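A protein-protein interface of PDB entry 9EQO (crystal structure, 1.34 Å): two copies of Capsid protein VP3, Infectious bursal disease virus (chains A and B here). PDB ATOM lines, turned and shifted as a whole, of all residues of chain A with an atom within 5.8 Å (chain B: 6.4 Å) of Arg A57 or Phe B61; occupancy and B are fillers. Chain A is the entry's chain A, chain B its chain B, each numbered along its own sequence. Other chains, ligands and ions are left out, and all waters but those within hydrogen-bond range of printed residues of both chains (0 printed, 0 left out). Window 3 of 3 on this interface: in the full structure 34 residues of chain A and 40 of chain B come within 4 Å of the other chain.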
ATOM      1  N   PHE A  48     -23.938 -14.857   4.575  1.00  0.00           N
ATOM      2  CA  PHE A  48     -23.668 -13.848   3.567  1.00  0.00           C
ATOM      3  C   PHE A  48     -24.397 -12.555   3.895  1.00  0.00           C
ATOM      4  O   PHE A  48     -23.841 -11.462   3.736  1.00  0.00           O
ATOM      5  CB  PHE A  48     -24.068 -14.344   2.182  1.00  0.00           C
ATOM      6  CG  PHE A  48     -23.835 -13.322   1.122  1.00  0.00           C
ATOM      7  CD1 PHE A  48     -22.608 -13.224   0.496  1.00  0.00           C
ATOM      8  CD2 PHE A  48     -24.824 -12.404   0.804  1.00  0.00           C
ATOM      9  CE1 PHE A  48     -22.394 -12.239  -0.466  1.00  0.00           C
ATOM     10  CE2 PHE A  48     -24.610 -11.432  -0.127  1.00  0.00           C
ATOM     11  CZ  PHE A  48     -23.406 -11.345  -0.764  1.00  0.00           C
ATOM     12  N   ASP A  52     -23.134  -8.667   4.032  1.00  0.00           N
ATOM     13  CA  ASP A  52     -23.679  -7.773   3.006  1.00  0.00           C
ATOM     14  C   ASP A  52     -25.045  -7.290   3.481  1.00  0.00           C
ATOM     15  O   ASP A  52     -26.077  -7.593   2.877  1.00  0.00           O
ATOM     16  CB  ASP A  52     -23.782  -8.539   1.685  1.00  0.00           C
ATOM     17  CG  ASP A  52     -24.134  -7.659   0.493  1.00  0.00           C
ATOM     18  OD1 ASP A  52     -23.655  -6.513   0.411  1.00  0.00           O
ATOM     19  OD2 ASP A  52     -24.859  -8.150  -0.399  1.00  0.00           O
ATOM     20  N   ALA A  55     -27.291  -5.612   1.052  1.00  0.00           N
ATOM     21  CA  ALA A  55     -27.465  -6.351  -0.192  1.00  0.00           C
ATOM     22  C   ALA A  55     -26.799  -5.670  -1.383  1.00  0.00           C
ATOM     23  O   ALA A  55     -27.175  -5.933  -2.524  1.00  0.00           O
ATOM     24  CB  ALA A  55     -28.939  -6.687  -0.483  1.00  0.00           C
ATOM     25  N   HIS A  56     -25.803  -4.813  -1.151  1.00  0.00           N
ATOM     26  CA  HIS A  56     -25.123  -4.165  -2.272  1.00  0.00           C
ATOM     27  C   HIS A  56     -24.479  -5.200  -3.186  1.00  0.00           C
ATOM     28  O   HIS A  56     -24.641  -5.164  -4.410  1.00  0.00           O
ATOM     29  CB  HIS A  56     -24.045  -3.203  -1.765  1.00  0.00           C
ATOM     30  CG  HIS A  56     -24.562  -2.020  -1.004  1.00  0.00           C
ATOM     31  ND1 HIS A  56     -25.704  -1.334  -1.358  1.00  0.00           N
ATOM     32  CD2 HIS A  56     -24.068  -1.390   0.088  1.00  0.00           C
ATOM     33  CE1 HIS A  56     -25.899  -0.339  -0.510  1.00  0.00           C
ATOM     34  NE2 HIS A  56     -24.918  -0.350   0.376  1.00  0.00           N
ATOM     35  N   ARG A  57     -23.726  -6.140  -2.603  1.00  0.00           N
ATOM     36  CA  ARG A  57     -23.045  -7.135  -3.421  1.00  0.00           C
ATOM     37  C   ARG A  57     -24.046  -8.097  -4.042  1.00  0.00           C
ATOM     38  O   ARG A  57     -23.927  -8.459  -5.220  1.00  0.00           O
ATOM     39  CB  ARG A  57     -22.003  -7.874  -2.581  1.00  0.00           C
ATOM     40  CG  ARG A  57     -21.107  -8.806  -3.373  1.00  0.00           C
ATOM     41  CD  ARG A  57     -19.958  -9.304  -2.514  1.00  0.00           C
ATOM     42  NE  ARG A  57     -18.980  -8.251  -2.281  1.00  0.00           N
ATOM     43  CZ  ARG A  57     -17.957  -7.991  -3.085  1.00  0.00           C
ATOM     44  NH1 ARG A  57     -17.738  -8.701  -4.180  1.00  0.00           N
ATOM     45  NH2 ARG A  57     -17.133  -6.988  -2.784  1.00  0.00           N
ATOM     46  N   MET A  58     -25.056  -8.502  -3.277  1.00  0.00           N
ATOM     47  CA  MET A  58     -26.041  -9.434  -3.809  1.00  0.00           C
ATOM     48  C   MET A  58     -26.848  -8.816  -4.943  1.00  0.00           C
ATOM     49  O   MET A  58     -27.111  -9.482  -5.950  1.00  0.00           O
ATOM     50  CB  MET A  58     -26.947  -9.951  -2.693  1.00  0.00           C
ATOM     51  CG  MET A  58     -27.968 -10.982  -3.182  1.00  0.00           C
ATOM     52  SD  MET A  58     -27.238 -12.481  -3.915  1.00  0.00           S
ATOM     53  CE  MET A  58     -26.738 -13.377  -2.451  1.00  0.00           C
ATOM     54  N   ARG A  59     -27.248  -7.545  -4.807  1.00  0.00           N
ATOM     55  CA  ARG A  59     -27.981  -6.882  -5.884  1.00  0.00           C
ATOM     56  C   ARG A  59     -27.192  -6.886  -7.186  1.00  0.00           C
ATOM     57  O   ARG A  59     -27.751  -7.151  -8.257  1.00  0.00           O
ATOM     58  CB  ARG A  59     -28.316  -5.444  -5.489  1.00  0.00           C
ATOM     59  CG  ARG A  59     -29.608  -5.299  -4.737  1.00  0.00           C
ATOM     60  CD  ARG A  59     -30.112  -3.850  -4.782  1.00  0.00           C
ATOM     61  NE  ARG A  59     -30.959  -3.557  -3.634  1.00  0.00           N
ATOM     62  CZ  ARG A  59     -30.499  -3.105  -2.474  1.00  0.00           C
ATOM     63  NH1 ARG A  59     -29.221  -2.796  -2.311  1.00  0.00           N
ATOM     64  NH2 ARG A  59     -31.334  -2.987  -1.447  1.00  0.00           N
ATOM     65  N   ASN A  60     -25.894  -6.579  -7.120  1.00  0.00           N
ATOM     66  CA  ASN A  60     -25.084  -6.552  -8.334  1.00  0.00           C
ATOM     67  C   ASN A  60     -25.018  -7.928  -8.975  1.00  0.00           C
ATOM     68  O   ASN A  60     -25.052  -8.051 -10.205  1.00  0.00           O
ATOM     69  CB  ASN A  60     -23.682  -6.035  -8.023  1.00  0.00           C
ATOM     70  CG  ASN A  60     -23.671  -4.558  -7.702  1.00  0.00           C
ATOM     71  OD1 ASN A  60     -24.610  -3.839  -8.034  1.00  0.00           O
ATOM     72  ND2 ASN A  60     -22.607  -4.096  -7.053  1.00  0.00           N
ATOM     73  N   PHE A  61     -24.934  -8.975  -8.153  1.00  0.00           N
ATOM     74  CA  PHE A  61     -24.882 -10.336  -8.671  1.00  0.00           C
ATOM     75  C   PHE A  61     -26.210 -10.727  -9.305  1.00  0.00           C
ATOM     76  O   PHE A  61     -26.241 -11.268 -10.417  1.00  0.00           O
ATOM     77  CB  PHE A  61     -24.518 -11.287  -7.532  1.00  0.00           C
ATOM     78  CG  PHE A  61     -24.462 -12.734  -7.924  1.00  0.00           C
ATOM     79  CD1 PHE A  61     -23.626 -13.163  -8.946  1.00  0.00           C
ATOM     80  CD2 PHE A  61     -25.215 -13.673  -7.245  1.00  0.00           C
ATOM     81  CE1 PHE A  61     -23.556 -14.500  -9.293  1.00  0.00           C
ATOM     82  CE2 PHE A  61     -25.141 -15.025  -7.584  1.00  0.00           C
ATOM     83  CZ  PHE A  61     -24.304 -15.431  -8.615  1.00  0.00           C
ATOM     84  N   LEU A  62     -27.318 -10.448  -8.621  1.00  0.00           N
ATOM     85  CA  LEU A  62     -28.614 -10.806  -9.183  1.00  0.00           C
ATOM     86  C   LEU A  62     -28.908 -10.019 -10.455  1.00  0.00           C
ATOM     87  O   LEU A  62     -29.518 -10.553 -11.390  1.00  0.00           O
ATOM     88  CB  LEU A  62     -29.714 -10.609  -8.137  1.00  0.00           C
ATOM     89  CG  LEU A  62     -29.594 -11.424  -6.845  1.00  0.00           C
ATOM     90  CD1 LEU A  62     -30.711 -11.052  -5.878  1.00  0.00           C
ATOM     91  CD2 LEU A  62     -29.601 -12.927  -7.121  1.00  0.00           C
ATOM     92  N   HIS B  56     -25.507 -24.191  -8.310  1.00  0.00           N
ATOM     93  CA  HIS B  56     -24.083 -24.161  -8.628  1.00  0.00           C
ATOM     94  C   HIS B  56     -23.567 -22.734  -8.717  1.00  0.00           C
ATOM     95  O   HIS B  56     -22.490 -22.419  -8.196  1.00  0.00           O
ATOM     96  CB  HIS B  56     -23.813 -24.915  -9.930  1.00  0.00           C
ATOM     97  CG  HIS B  56     -24.054 -26.388  -9.832  1.00  0.00           C
ATOM     98  ND1 HIS B  56     -23.391 -27.190  -8.927  1.00  0.00           N
ATOM     99  CD2 HIS B  56     -24.891 -27.203 -10.514  1.00  0.00           C
ATOM    100  CE1 HIS B  56     -23.805 -28.437  -9.062  1.00  0.00           C
ATOM    101  NE2 HIS B  56     -24.716 -28.472 -10.018  1.00  0.00           N
ATOM    102  N   ARG B  57     -24.337 -21.842  -9.347  1.00  0.00           N
ATOM    103  CA  ARG B  57     -23.889 -20.455  -9.451  1.00  0.00           C
ATOM    104  C   ARG B  57     -23.939 -19.763  -8.097  1.00  0.00           C
ATOM    105  O   ARG B  57     -23.011 -19.032  -7.724  1.00  0.00           O
ATOM    106  CB  ARG B  57     -24.738 -19.706 -10.473  1.00  0.00           C
ATOM    107  CG  ARG B  57     -24.621 -20.252 -11.881  1.00  0.00           C
ATOM    108  CD  ARG B  57     -25.763 -19.736 -12.733  1.00  0.00           C
ATOM    109  NE  ARG B  57     -25.796 -20.366 -14.046  1.00  0.00           N
ATOM    110  CZ  ARG B  57     -26.385 -21.524 -14.313  1.00  0.00           C
ATOM    111  NH1 ARG B  57     -27.017 -22.209 -13.373  1.00  0.00           N
ATOM    112  NH2 ARG B  57     -26.332 -22.007 -15.552  1.00  0.00           N
ATOM    113  N   MET B  58     -25.002 -19.997  -7.333  1.00  0.00           N
ATOM    114  CA  MET B  58     -25.080 -19.355  -6.029  1.00  0.00           C
ATOM    115  C   MET B  58     -24.017 -19.885  -5.068  1.00  0.00           C
ATOM    116  O   MET B  58     -23.438 -19.109  -4.308  1.00  0.00           O
ATOM    117  CB  MET B  58     -26.492 -19.460  -5.461  1.00  0.00           C
ATOM    118  CG  MET B  58     -26.639 -18.700  -4.140  1.00  0.00           C
ATOM    119  SD  MET B  58     -26.302 -16.921  -4.212  1.00  0.00           S
ATOM    120  CE  MET B  58     -27.833 -16.282  -4.897  1.00  0.00           C
ATOM    121  N   ARG B  59     -23.752 -21.200  -5.075  1.00  0.00           N
ATOM    122  CA  ARG B  59     -22.706 -21.730  -4.199  1.00  0.00           C
ATOM    123  C   ARG B  59     -21.360 -21.114  -4.535  1.00  0.00           C
ATOM    124  O   ARG B  59     -20.592 -20.750  -3.642  1.00  0.00           O
ATOM    125  CB  ARG B  59     -22.601 -23.244  -4.345  1.00  0.00           C
ATOM    126  CG  ARG B  59     -23.663 -24.019  -3.592  1.00  0.00           C
ATOM    127  CD  ARG B  59     -23.262 -25.484  -3.492  1.00  0.00           C
ATOM    128  NE  ARG B  59     -24.415 -26.329  -3.221  1.00  0.00           N
ATOM    129  CZ  ARG B  59     -25.214 -26.799  -4.166  1.00  0.00           C
ATOM    130  NH1 ARG B  59     -24.960 -26.592  -5.449  1.00  0.00           N
ATOM    131  NH2 ARG B  59     -26.309 -27.471  -3.817  1.00  0.00           N
ATOM    132  N   ASN B  60     -21.068 -20.973  -5.824  1.00  0.00           N
ATOM    133  CA  ASN B  60     -19.811 -20.362  -6.232  1.00  0.00           C
ATOM    134  C   ASN B  60     -19.709 -18.929  -5.729  1.00  0.00           C
ATOM    135  O   ASN B  60     -18.648 -18.489  -5.270  1.00  0.00           O
ATOM    136  CB  ASN B  60     -19.700 -20.418  -7.751  1.00  0.00           C
ATOM    137  CG  ASN B  60     -18.428 -19.798  -8.254  1.00  0.00           C
ATOM    138  OD1 ASN B  60     -17.332 -20.256  -7.920  1.00  0.00           O
ATOM    139  ND2 ASN B  60     -18.555 -18.767  -9.076  1.00  0.00           N
ATOM    140  N   PHE B  61     -20.811 -18.190  -5.791  1.00  0.00           N
ATOM    141  CA  PHE B  61     -20.827 -16.814  -5.314  1.00  0.00           C
ATOM    142  C   PHE B  61     -20.652 -16.746  -3.798  1.00  0.00           C
ATOM    143  O   PHE B  61     -19.880 -15.924  -3.293  1.00  0.00           O
ATOM    144  CB  PHE B  61     -22.146 -16.174  -5.738  1.00  0.00           C
ATOM    145  CG  PHE B  61     -22.294 -14.757  -5.309  1.00  0.00           C
ATOM    146  CD1 PHE B  61     -21.608 -13.753  -5.964  1.00  0.00           C
ATOM    147  CD2 PHE B  61     -23.129 -14.429  -4.256  1.00  0.00           C
ATOM    148  CE1 PHE B  61     -21.743 -12.442  -5.576  1.00  0.00           C
ATOM    149  CE2 PHE B  61     -23.272 -13.114  -3.868  1.00  0.00           C
ATOM    150  CZ  PHE B  61     -22.575 -12.119  -4.531  1.00  0.00           C
ATOM    151  N   LEU B  62     -21.360 -17.601  -3.058  1.00  0.00           N
ATOM    152  CA  LEU B  62     -21.277 -17.572  -1.599  1.00  0.00           C
ATOM    153  C   LEU B  62     -19.909 -18.012  -1.104  1.00  0.00           C
ATOM    154  O   LEU B  62     -19.453 -17.547  -0.058  1.00  0.00           O
ATOM    155  CB  LEU B  62     -22.346 -18.481  -1.008  1.00  0.00           C
ATOM    156  CG  LEU B  62     -23.790 -18.030  -1.222  1.00  0.00           C
ATOM    157  CD1 LEU B  62     -24.751 -19.118  -0.750  1.00  0.00           C
ATOM    158  CD2 LEU B  62     -24.048 -16.721  -0.505  1.00  0.00           C
ATOM    159  N   ALA B  63     -19.254 -18.903  -1.839  1.00  0.00           N
ATOM    160  CA  ALA B  63     -17.981 -19.451  -1.390  1.00  0.00           C
ATOM    161  C   ALA B  63     -16.899 -18.385  -1.328  1.00  0.00           C
ATOM    162  O   ALA B  63     -15.979 -18.481  -0.512  1.00  0.00           O
ATOM    163  CB  ALA B  63     -17.556 -20.574  -2.333  1.00  0.00           C
ATOM    164  N   ASN B  64     -16.994 -17.362  -2.170  1.00  0.00           N
ATOM    165  CA  ASN B  64     -15.908 -16.415  -2.354  1.00  0.00           C
ATOM    166  C   ASN B  64     -16.268 -15.005  -1.916  1.00  0.00           C
ATOM    167  O   ASN B  64     -15.512 -14.070  -2.202  1.00  0.00           O
ATOM    168  CB  ASN B  64     -15.450 -16.434  -3.808  1.00  0.00           C
ATOM    169  CG  ASN B  64     -14.887 -17.779  -4.218  1.00  0.00           C
ATOM    170  OD1 ASN B  64     -13.734 -18.097  -3.918  1.00  0.00           O
ATOM    171  ND2 ASN B  64     -15.698 -18.580  -4.904  1.00  0.00           N
ATOM    172  N   ALA B  65     -17.383 -14.830  -1.223  1.00  0.00           N
ATOM    173  CA  ALA B  65     -17.784 -13.521  -0.741  1.00  0.00           C
ATOM    174  C   ALA B  65     -16.967 -13.130   0.488  1.00  0.00           C
ATOM    175  O   ALA B  65     -16.589 -11.963   0.649  1.00  0.00           O
ATOM    176  CB  ALA B  65     -19.258 -13.522  -0.414  1.00  0.00           C
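The side-chain carboxylate (OD2) of Asp A52 is in hydrogen-bond range of the backbone NH (N) of Met A58.
The side-chain carboxylate of Asp A52 is in hydrogen-bond range of the backbone NH of Arg A57 (3.0 Å).
Among the printed residues, pairs that only touch across the chains: Phe A48 with Ala B65 (3.4 Å), Phe A48 with Phe B61 (3.6 Å), Phe A61 with Phe B61 (3.6 Å), Phe A48 with Leu B62 (3.6 Å), Met A58 with Phe B61 (3.8 Å), Arg A57 with Phe B61 (3.8 Å), Phe A61 with Arg B57 (3.9 Å) and Met A58 with Met B58 (3.95 Å).
Of the printed residues of chain B, Phe A48 touches Phe B61, Leu B62 and Ala B65.
His A56 touches none of the printed residues of chain B.
Of chain B, only Phe B61 (3.8 Å) comes within 4 Å of Arg A57.
Printed residues of chain A within 4 Å of Arg B57: Phe A61.
Phe B61 touches four residues of chain A.
The nearest printed residue of chain A that does not touch Phe B61 is Asp A52 (6.2 Å).
Printed residues of chain B that touch a printed residue of chain A: Arg B57, Met B58, Phe B61, Leu B62 and Ala B65.
Among the printed residues, 8 pairs touch across the chains.
Arg A57 touches Phe B61, and with the chains exchanged Phe A61 touches Arg B57.
Met A58 touches its own counterpart, Met B58.
Met A58 touches Phe B61, but with the chains exchanged Phe A61 does not touch Met B58 (4.01 Å).
Phe B61 touches its own counterpart, Phe A61.
7 positions are printed for both chains.
Of the 8 pairs that touch across the chains among the printed residues, 4 have their exchanged pair printed and touching as well.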
